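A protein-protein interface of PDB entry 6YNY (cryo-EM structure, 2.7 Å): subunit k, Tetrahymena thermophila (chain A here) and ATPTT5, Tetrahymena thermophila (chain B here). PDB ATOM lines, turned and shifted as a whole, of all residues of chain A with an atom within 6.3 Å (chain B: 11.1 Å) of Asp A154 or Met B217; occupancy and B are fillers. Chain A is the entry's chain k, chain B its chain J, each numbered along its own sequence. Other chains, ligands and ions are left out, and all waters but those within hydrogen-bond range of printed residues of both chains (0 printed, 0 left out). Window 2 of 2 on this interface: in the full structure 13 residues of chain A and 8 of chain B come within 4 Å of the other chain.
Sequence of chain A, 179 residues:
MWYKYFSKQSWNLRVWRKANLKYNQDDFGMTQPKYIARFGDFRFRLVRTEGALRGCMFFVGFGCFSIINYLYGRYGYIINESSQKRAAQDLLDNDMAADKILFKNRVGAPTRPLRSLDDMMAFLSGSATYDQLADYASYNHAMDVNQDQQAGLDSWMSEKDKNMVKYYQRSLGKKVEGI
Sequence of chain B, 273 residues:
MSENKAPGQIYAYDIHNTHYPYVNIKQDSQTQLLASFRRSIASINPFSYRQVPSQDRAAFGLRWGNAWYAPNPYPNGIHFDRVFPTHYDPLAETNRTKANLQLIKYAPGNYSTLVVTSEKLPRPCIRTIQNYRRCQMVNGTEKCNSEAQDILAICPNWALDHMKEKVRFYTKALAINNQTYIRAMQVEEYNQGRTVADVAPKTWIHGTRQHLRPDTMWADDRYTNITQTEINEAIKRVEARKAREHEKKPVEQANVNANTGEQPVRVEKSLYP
Hydrophobic or aromatic side chains of chain A within 4 Å of the printed part of chain B: Trp A156. Along chain A the printed residues that touch a printed residue of chain B span positions 152 to 156. Among the printed residues, 5 pairs touch across the chains. Among the printed residues, no Asp or Glu carboxylate lies within 4 Å of a Lys or Arg side-chain nitrogen of the other chain.
No residue of chain B comes within 4 Å of Gln A149. Gly A152 touches one residue of chain B. No residue of chain B comes within 4 Å of Leu A153. Of chain B, only Thr B216 and Met B217 come within 4 Å of Asp A154. Of chain B, only Asp B215 (3.0 Å) comes within 4 Å of Ser A155. Printed residues of chain B within 4 Å of Trp A156: Asp B215. Of the printed residues of chain A, Asp B215 touches Ser A155 (3.0 Å) and Trp A156 (3.1 Å). Of the printed residues of chain A, Thr B216 touches Asp A154 (3.5 Å). Met B217 touches one residue of chain A. Of the printed residues of chain A, Trp B218 touches Gly A152 (3.4 Å). Ile B231 touches none of the printed residues of chain A. The nearest residue of chain A that does not touch Met B217 is Ser A155 (4.1 Å).
Among the printed residues, pairs that only touch across the chains: Gly A152 with Trp B218 and Asp A154 with Thr B216.
NH1 of Arg B213 sits close to O of Thr B216. NH2 of Arg A106 lies within hydrogen-bond range of O of Ser A155, at 2.5 Å. The side-chain carboxylate (OD1) of Asp A154 lies within salt-bridge range of the guanidinium group (NH1) of Arg A106 (2.8 Å). The side-chain sulfur (SD) of Met B217 sits at hydrogen-bond distance from the indole nitrogen (NE1) of Trp B218 (3.1 Å).
The side-chain hydroxyl (OG) of Ser A155 sits at hydrogen-bond distance from the backbone carbonyl oxygen (O) of Asp B215 (3.0 Å). The side-chain carboxylate of Asp B215 sits at hydrogen-bond distance from the indole nitrogen of Trp A156 (3.1 Å). The backbone NH (N) of Met B217 sits at hydrogen-bond distance from the backbone carbonyl oxygen (O) of Asp A154 (3.2 Å).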
ATOM      1  N   ARG A 106     -23.181  27.475  19.450  1.00  0.00           N
ATOM      2  CA  ARG A 106     -23.512  28.583  18.565  1.00  0.00           C
ATOM      3  C   ARG A 106     -25.015  28.744  18.390  1.00  0.00           C
ATOM      4  O   ARG A 106     -25.470  29.819  17.986  1.00  0.00           O
ATOM      5  CB  ARG A 106     -22.815  28.385  17.225  1.00  0.00           C
ATOM      6  CG  ARG A 106     -21.316  28.585  17.325  1.00  0.00           C
ATOM      7  CD  ARG A 106     -20.606  28.361  16.011  1.00  0.00           C
ATOM      8  NE  ARG A 106     -20.593  26.958  15.622  1.00  0.00           N
ATOM      9  CZ  ARG A 106     -20.093  26.513  14.477  1.00  0.00           C
ATOM     10  NH1 ARG A 106     -20.118  25.221  14.201  1.00  0.00           N
ATOM     11  NH2 ARG A 106     -19.572  27.361  13.607  1.00  0.00           N
ATOM     12  N   ASP A 148     -22.102  16.888   9.705  1.00  0.00           N
ATOM     13  CA  ASP A 148     -21.053  17.406   8.835  1.00  0.00           C
ATOM     14  C   ASP A 148     -19.881  17.944   9.645  1.00  0.00           C
ATOM     15  O   ASP A 148     -18.718  17.737   9.280  1.00  0.00           O
ATOM     16  CB  ASP A 148     -21.621  18.496   7.931  1.00  0.00           C
ATOM     17  CG  ASP A 148     -22.572  17.949   6.890  1.00  0.00           C
ATOM     18  OD1 ASP A 148     -23.445  17.134   7.248  1.00  0.00           O
ATOM     19  OD2 ASP A 148     -22.454  18.341   5.711  1.00  0.00           O
ATOM     20  N   GLN A 149     -20.167  18.643  10.744  1.00  0.00           N
ATOM     21  CA  GLN A 149     -19.096  19.161  11.586  1.00  0.00           C
ATOM     22  C   GLN A 149     -18.237  18.032  12.132  1.00  0.00           C
ATOM     23  O   GLN A 149     -17.006  18.142  12.176  1.00  0.00           O
ATOM     24  CB  GLN A 149     -19.681  19.979  12.733  1.00  0.00           C
ATOM     25  CG  GLN A 149     -20.492  21.171  12.299  1.00  0.00           C
ATOM     26  CD  GLN A 149     -21.223  21.815  13.450  1.00  0.00           C
ATOM     27  OE1 GLN A 149     -21.286  21.264  14.547  1.00  0.00           O
ATOM     28  NE2 GLN A 149     -21.779  22.992  13.209  1.00  0.00           N
ATOM     29  N   GLY A 152     -15.765  17.033   9.619  1.00  0.00           N
ATOM     30  CA  GLY A 152     -14.717  17.989   9.326  1.00  0.00           C
ATOM     31  C   GLY A 152     -15.153  19.223   8.567  1.00  0.00           C
ATOM     32  O   GLY A 152     -14.312  20.040   8.187  1.00  0.00           O
ATOM     33  N   LEU A 153     -16.452  19.377   8.334  1.00  0.00           N
ATOM     34  CA  LEU A 153     -16.980  20.524   7.606  1.00  0.00           C
ATOM     35  C   LEU A 153     -17.612  21.488   8.601  1.00  0.00           C
ATOM     36  O   LEU A 153     -18.709  21.237   9.109  1.00  0.00           O
ATOM     37  CB  LEU A 153     -17.994  20.083   6.555  1.00  0.00           C
ATOM     38  CG  LEU A 153     -18.507  21.180   5.627  1.00  0.00           C
ATOM     39  CD1 LEU A 153     -17.389  21.702   4.767  1.00  0.00           C
ATOM     40  CD2 LEU A 153     -19.635  20.670   4.767  1.00  0.00           C
ATOM     41  N   ASP A 154     -16.923  22.592   8.872  1.00  0.00           N
ATOM     42  CA  ASP A 154     -17.431  23.603   9.783  1.00  0.00           C
ATOM     43  C   ASP A 154     -16.977  24.967   9.290  1.00  0.00           C
ATOM     44  O   ASP A 154     -16.005  25.084   8.540  1.00  0.00           O
ATOM     45  CB  ASP A 154     -16.958  23.358  11.218  1.00  0.00           C
ATOM     46  CG  ASP A 154     -17.702  24.195  12.228  1.00  0.00           C
ATOM     47  OD1 ASP A 154     -18.640  24.915  11.830  1.00  0.00           O
ATOM     48  OD2 ASP A 154     -17.352  24.134  13.424  1.00  0.00           O
ATOM     49  N   SER A 155     -17.695  25.997   9.715  1.00  0.00           N
ATOM     50  CA  SER A 155     -17.393  27.361   9.310  1.00  0.00           C
ATOM     51  C   SER A 155     -18.055  28.314  10.295  1.00  0.00           C
ATOM     52  O   SER A 155     -18.565  27.901  11.342  1.00  0.00           O
ATOM     53  CB  SER A 155     -17.857  27.616   7.874  1.00  0.00           C
ATOM     54  OG  SER A 155     -17.570  28.941   7.472  1.00  0.00           O
ATOM     55  N   TRP A 156     -18.039  29.599   9.961  1.00  0.00           N
ATOM     56  CA  TRP A 156     -18.663  30.606  10.798  1.00  0.00           C
ATOM     57  C   TRP A 156     -20.160  30.670  10.518  1.00  0.00           C
ATOM     58  O   TRP A 156     -20.642  30.265   9.458  1.00  0.00           O
ATOM     59  CB  TRP A 156     -18.018  31.972  10.571  1.00  0.00           C
ATOM     60  CG  TRP A 156     -18.054  32.435   9.157  1.00  0.00           C
ATOM     61  CD1 TRP A 156     -17.128  32.186   8.192  1.00  0.00           C
ATOM     62  CD2 TRP A 156     -19.066  33.238   8.544  1.00  0.00           C
ATOM     63  NE1 TRP A 156     -17.500  32.779   7.014  1.00  0.00           N
ATOM     64  CE2 TRP A 156     -18.688  33.432   7.204  1.00  0.00           C
ATOM     65  CE3 TRP A 156     -20.255  33.810   8.999  1.00  0.00           C
ATOM     66  CZ2 TRP A 156     -19.456  34.173   6.315  1.00  0.00           C
ATOM     67  CZ3 TRP A 156     -21.016  34.545   8.115  1.00  0.00           C
ATOM     68  CH2 TRP A 156     -20.614  34.720   6.789  1.00  0.00           C
ATOM     69  N   MET A 157     -20.898  31.192  11.492  1.00  0.00           N
ATOM     70  CA  MET A 157     -22.348  31.240  11.440  1.00  0.00           C
ATOM     71  C   MET A 157     -22.824  32.680  11.543  1.00  0.00           C
ATOM     72  O   MET A 157     -22.317  33.458  12.356  1.00  0.00           O
ATOM     73  CB  MET A 157     -22.961  30.409  12.567  1.00  0.00           C
ATOM     74  CG  MET A 157     -22.596  28.946  12.505  1.00  0.00           C
ATOM     75  SD  MET A 157     -23.202  27.982  13.897  1.00  0.00           S
ATOM     76  CE  MET A 157     -24.958  28.218  13.721  1.00  0.00           C
ATOM     77  N   ARG B 209      -8.281  25.295  -4.350  1.00  0.00           N
ATOM     78  CA  ARG B 209      -8.030  25.095  -2.927  1.00  0.00           C
ATOM     79  C   ARG B 209      -6.559  25.250  -2.568  1.00  0.00           C
ATOM     80  O   ARG B 209      -6.237  25.617  -1.433  1.00  0.00           O
ATOM     81  CB  ARG B 209      -8.543  23.718  -2.514  1.00  0.00           C
ATOM     82  CG  ARG B 209      -8.085  23.250  -1.156  1.00  0.00           C
ATOM     83  CD  ARG B 209      -8.919  22.082  -0.687  1.00  0.00           C
ATOM     84  NE  ARG B 209      -8.942  20.993  -1.656  1.00  0.00           N
ATOM     85  CZ  ARG B 209      -8.058  20.004  -1.698  1.00  0.00           C
ATOM     86  NH1 ARG B 209      -7.060  19.954  -0.830  1.00  0.00           N
ATOM     87  NH2 ARG B 209      -8.171  19.060  -2.618  1.00  0.00           N
ATOM     88  N   ARG B 213      -7.745  29.783  -0.262  1.00  0.00           N
ATOM     89  CA  ARG B 213      -8.283  28.985   0.827  1.00  0.00           C
ATOM     90  C   ARG B 213      -9.804  29.055   0.819  1.00  0.00           C
ATOM     91  O   ARG B 213     -10.366  30.150   0.710  1.00  0.00           O
ATOM     92  CB  ARG B 213      -7.751  29.477   2.165  1.00  0.00           C
ATOM     93  CG  ARG B 213      -7.673  28.397   3.219  1.00  0.00           C
ATOM     94  CD  ARG B 213      -7.433  28.977   4.587  1.00  0.00           C
ATOM     95  NE  ARG B 213      -8.683  29.207   5.300  1.00  0.00           N
ATOM     96  CZ  ARG B 213      -9.244  28.330   6.125  1.00  0.00           C
ATOM     97  NH1 ARG B 213      -8.675  27.157   6.355  1.00  0.00           N
ATOM     98  NH2 ARG B 213     -10.383  28.629   6.727  1.00  0.00           N
ATOM     99  N   PRO B 214     -10.505  27.930   0.930  1.00  0.00           N
ATOM    100  CA  PRO B 214     -11.964  27.985   1.029  1.00  0.00           C
ATOM    101  C   PRO B 214     -12.407  28.678   2.307  1.00  0.00           C
ATOM    102  O   PRO B 214     -11.618  28.963   3.209  1.00  0.00           O
ATOM    103  CB  PRO B 214     -12.383  26.513   1.014  1.00  0.00           C
ATOM    104  CG  PRO B 214     -11.227  25.784   0.464  1.00  0.00           C
ATOM    105  CD  PRO B 214     -10.019  26.543   0.859  1.00  0.00           C
ATOM    106  N   ASP B 215     -13.704  28.952   2.375  1.00  0.00           N
ATOM    107  CA  ASP B 215     -14.304  29.601   3.538  1.00  0.00           C
ATOM    108  C   ASP B 215     -14.751  28.575   4.576  1.00  0.00           C
ATOM    109  O   ASP B 215     -15.899  28.561   5.015  1.00  0.00           O
ATOM    110  CB  ASP B 215     -15.467  30.478   3.099  1.00  0.00           C
ATOM    111  CG  ASP B 215     -15.957  31.390   4.200  1.00  0.00           C
ATOM    112  OD1 ASP B 215     -15.381  31.353   5.306  1.00  0.00           O
ATOM    113  OD2 ASP B 215     -16.919  32.148   3.961  1.00  0.00           O
ATOM    114  N   THR B 216     -13.830  27.698   4.967  1.00  0.00           N
ATOM    115  CA  THR B 216     -14.079  26.713   6.006  1.00  0.00           C
ATOM    116  C   THR B 216     -12.861  26.638   6.913  1.00  0.00           C
ATOM    117  O   THR B 216     -11.731  26.881   6.481  1.00  0.00           O
ATOM    118  CB  THR B 216     -14.386  25.333   5.417  1.00  0.00           C
ATOM    119  OG1 THR B 216     -13.323  24.928   4.550  1.00  0.00           O
ATOM    120  CG2 THR B 216     -15.680  25.370   4.635  1.00  0.00           C
ATOM    121  N   MET B 217     -13.103  26.298   8.180  1.00  0.00           N
ATOM    122  CA  MET B 217     -12.039  26.341   9.176  1.00  0.00           C
ATOM    123  C   MET B 217     -11.085  25.161   9.071  1.00  0.00           C
ATOM    124  O   MET B 217      -9.899  25.306   9.387  1.00  0.00           O
ATOM    125  CB  MET B 217     -12.637  26.390  10.582  1.00  0.00           C
ATOM    126  CG  MET B 217     -13.608  25.282  10.875  1.00  0.00           C
ATOM    127  SD  MET B 217     -14.107  25.223  12.605  1.00  0.00           S
ATOM    128  CE  MET B 217     -14.918  26.802  12.771  1.00  0.00           C
ATOM    129  N   TRP B 218     -11.563  24.001   8.628  1.00  0.00           N
ATOM    130  CA  TRP B 218     -10.748  22.795   8.585  1.00  0.00           C
ATOM    131  C   TRP B 218     -10.349  22.414   7.166  1.00  0.00           C
ATOM    132  O   TRP B 218     -10.074  21.243   6.894  1.00  0.00           O
ATOM    133  CB  TRP B 218     -11.478  21.639   9.263  1.00  0.00           C
ATOM    134  CG  TRP B 218     -11.959  21.970  10.633  1.00  0.00           C
ATOM    135  CD1 TRP B 218     -13.207  21.761  11.133  1.00  0.00           C
ATOM    136  CD2 TRP B 218     -11.206  22.587  11.682  1.00  0.00           C
ATOM    137  NE1 TRP B 218     -13.279  22.203  12.428  1.00  0.00           N
ATOM    138  CE2 TRP B 218     -12.062  22.713  12.790  1.00  0.00           C
ATOM    139  CE3 TRP B 218      -9.891  23.041  11.793  1.00  0.00           C
ATOM    140  CZ2 TRP B 218     -11.645  23.277  13.989  1.00  0.00           C
ATOM    141  CZ3 TRP B 218      -9.483  23.596  12.984  1.00  0.00           C
ATOM    142  CH2 TRP B 218     -10.354  23.710  14.065  1.00  0.00           C
ATOM    143  N   ALA B 219     -10.312  23.387   6.255  1.00  0.00           N
ATOM    144  CA  ALA B 219      -9.813  23.120   4.913  1.00  0.00           C
ATOM    145  C   ALA B 219      -8.315  22.858   4.920  1.00  0.00           C
ATOM    146  O   ALA B 219      -7.823  22.056   4.119  1.00  0.00           O
ATOM    147  CB  ALA B 219     -10.136  24.292   3.993  1.00  0.00           C
ATOM    148  N   ASP B 220      -7.583  23.520   5.809  1.00  0.00           N
ATOM    149  CA  ASP B 220      -6.148  23.332   5.944  1.00  0.00           C
ATOM    150  C   ASP B 220      -5.801  23.417   7.426  1.00  0.00           C
ATOM    151  O   ASP B 220      -6.679  23.382   8.293  1.00  0.00           O
ATOM    152  CB  ASP B 220      -5.389  24.359   5.095  1.00  0.00           C
ATOM    153  CG  ASP B 220      -5.730  25.787   5.463  1.00  0.00           C
ATOM    154  OD1 ASP B 220      -6.612  25.988   6.323  1.00  0.00           O
ATOM    155  OD2 ASP B 220      -5.116  26.709   4.889  1.00  0.00           O
ATOM    156  N   ASP B 221      -4.505  23.532   7.720  1.00  0.00           N
ATOM    157  CA  ASP B 221      -4.003  23.573   9.088  1.00  0.00           C
ATOM    158  C   ASP B 221      -3.839  24.994   9.614  1.00  0.00           C
ATOM    159  O   ASP B 221      -2.925  25.259  10.406  1.00  0.00           O
ATOM    160  CB  ASP B 221      -2.676  22.817   9.176  1.00  0.00           C
ATOM    161  CG  ASP B 221      -1.676  23.268   8.132  1.00  0.00           C
ATOM    162  OD1 ASP B 221      -1.361  24.475   8.087  1.00  0.00           O
ATOM    163  OD2 ASP B 221      -1.205  22.414   7.353  1.00  0.00           O
ATOM    164  N   ARG B 222      -4.707  25.916   9.200  1.00  0.00           N
ATOM    165  CA  ARG B 222      -4.558  27.310   9.601  1.00  0.00           C
ATOM    166  C   ARG B 222      -4.931  27.515  11.065  1.00  0.00           C
ATOM    167  O   ARG B 222      -4.212  28.194  11.807  1.00  0.00           O
ATOM    168  CB  ARG B 222      -5.415  28.199   8.702  1.00  0.00           C
ATOM    169  CG  ARG B 222      -5.278  29.676   8.981  1.00  0.00           C
ATOM    170  CD  ARG B 222      -6.132  30.501   8.046  1.00  0.00           C
ATOM    171  NE  ARG B 222      -6.017  31.927   8.325  1.00  0.00           N
ATOM    172  CZ  ARG B 222      -5.069  32.716   7.832  1.00  0.00           C
ATOM    173  NH1 ARG B 222      -4.140  32.227   7.024  1.00  0.00           N
ATOM    174  NH2 ARG B 222      -5.053  33.999   8.152  1.00  0.00           N
ATOM    175  N   TYR B 223      -6.054  26.943  11.498  1.00  0.00           N
ATOM    176  CA  TYR B 223      -6.565  27.145  12.848  1.00  0.00           C
ATOM    177  C   TYR B 223      -6.372  25.917  13.733  1.00  0.00           C
ATOM    178  O   TYR B 223      -7.116  25.719  14.696  1.00  0.00           O
ATOM    179  CB  TYR B 223      -8.044  27.517  12.804  1.00  0.00           C
ATOM    180  CG  TYR B 223      -8.364  28.678  11.897  1.00  0.00           C
ATOM    181  CD1 TYR B 223      -8.089  29.978  12.278  1.00  0.00           C
ATOM    182  CD2 TYR B 223      -8.955  28.471  10.663  1.00  0.00           C
ATOM    183  CE1 TYR B 223      -8.385  31.037  11.454  1.00  0.00           C
ATOM    184  CE2 TYR B 223      -9.254  29.523   9.833  1.00  0.00           C
ATOM    185  CZ  TYR B 223      -8.967  30.804  10.233  1.00  0.00           C
ATOM    186  OH  TYR B 223      -9.261  31.859   9.409  1.00  0.00           O
ATOM    187  N   THR B 224      -5.378  25.085  13.427  1.00  0.00           N
ATOM    188  CA  THR B 224      -5.157  23.875  14.207  1.00  0.00           C
ATOM    189  C   THR B 224      -4.383  24.127  15.492  1.00  0.00           C
ATOM    190  O   THR B 224      -4.415  23.280  16.391  1.00  0.00           O
ATOM    191  CB  THR B 224      -4.416  22.837  13.366  1.00  0.00           C
ATOM    192  OG1 THR B 224      -3.203  23.401  12.859  1.00  0.00           O
ATOM    193  CG2 THR B 224      -5.281  22.386  12.214  1.00  0.00           C
ATOM    194  N   ASN B 225      -3.691  25.260  15.603  1.00  0.00           N
ATOM    195  CA  ASN B 225      -2.925  25.599  16.793  1.00  0.00           C
ATOM    196  C   ASN B 225      -3.615  26.654  17.647  1.00  0.00           C
ATOM    197  O   ASN B 225      -2.947  27.364  18.406  1.00  0.00           O
ATOM    198  CB  ASN B 225      -1.530  26.075  16.398  1.00  0.00           C
ATOM    199  CG  ASN B 225      -0.743  25.016  15.659  1.00  0.00           C
ATOM    200  OD1 ASN B 225      -1.033  23.825  15.763  1.00  0.00           O
ATOM    201  ND2 ASN B 225       0.266  25.443  14.911  1.00  0.00           N
ATOM    202  N   ILE B 226      -4.929  26.770  17.542  1.00  0.00           N
ATOM    203  CA  ILE B 226      -5.689  27.765  18.287  1.00  0.00           C
ATOM    204  C   ILE B 226      -6.146  27.160  19.605  1.00  0.00           C
ATOM    205  O   ILE B 226      -6.603  26.013  19.655  1.00  0.00           O
ATOM    206  CB  ILE B 226      -6.887  28.263  17.460  1.00  0.00           C
ATOM    207  CG1 ILE B 226      -6.414  28.859  16.135  1.00  0.00           C
ATOM    208  CG2 ILE B 226      -7.679  29.287  18.240  1.00  0.00           C
ATOM    209  CD1 ILE B 226      -5.506  30.052  16.278  1.00  0.00           C
ATOM    210  N   ILE B 231      -9.527  32.084  21.651  1.00  0.00           N
ATOM    211  CA  ILE B 231     -10.918  32.186  21.226  1.00  0.00           C
ATOM    212  C   ILE B 231     -11.657  33.218  22.065  1.00  0.00           C
ATOM    213  O   ILE B 231     -12.342  34.099  21.532  1.00  0.00           O
ATOM    214  CB  ILE B 231     -11.598  30.809  21.304  1.00  0.00           C
ATOM    215  CG1 ILE B 231     -10.940  29.841  20.325  1.00  0.00           C
ATOM    216  CG2 ILE B 231     -13.077  30.938  21.019  1.00  0.00           C
ATOM    217  CD1 ILE B 231     -11.398  28.421  20.475  1.00  0.00           C
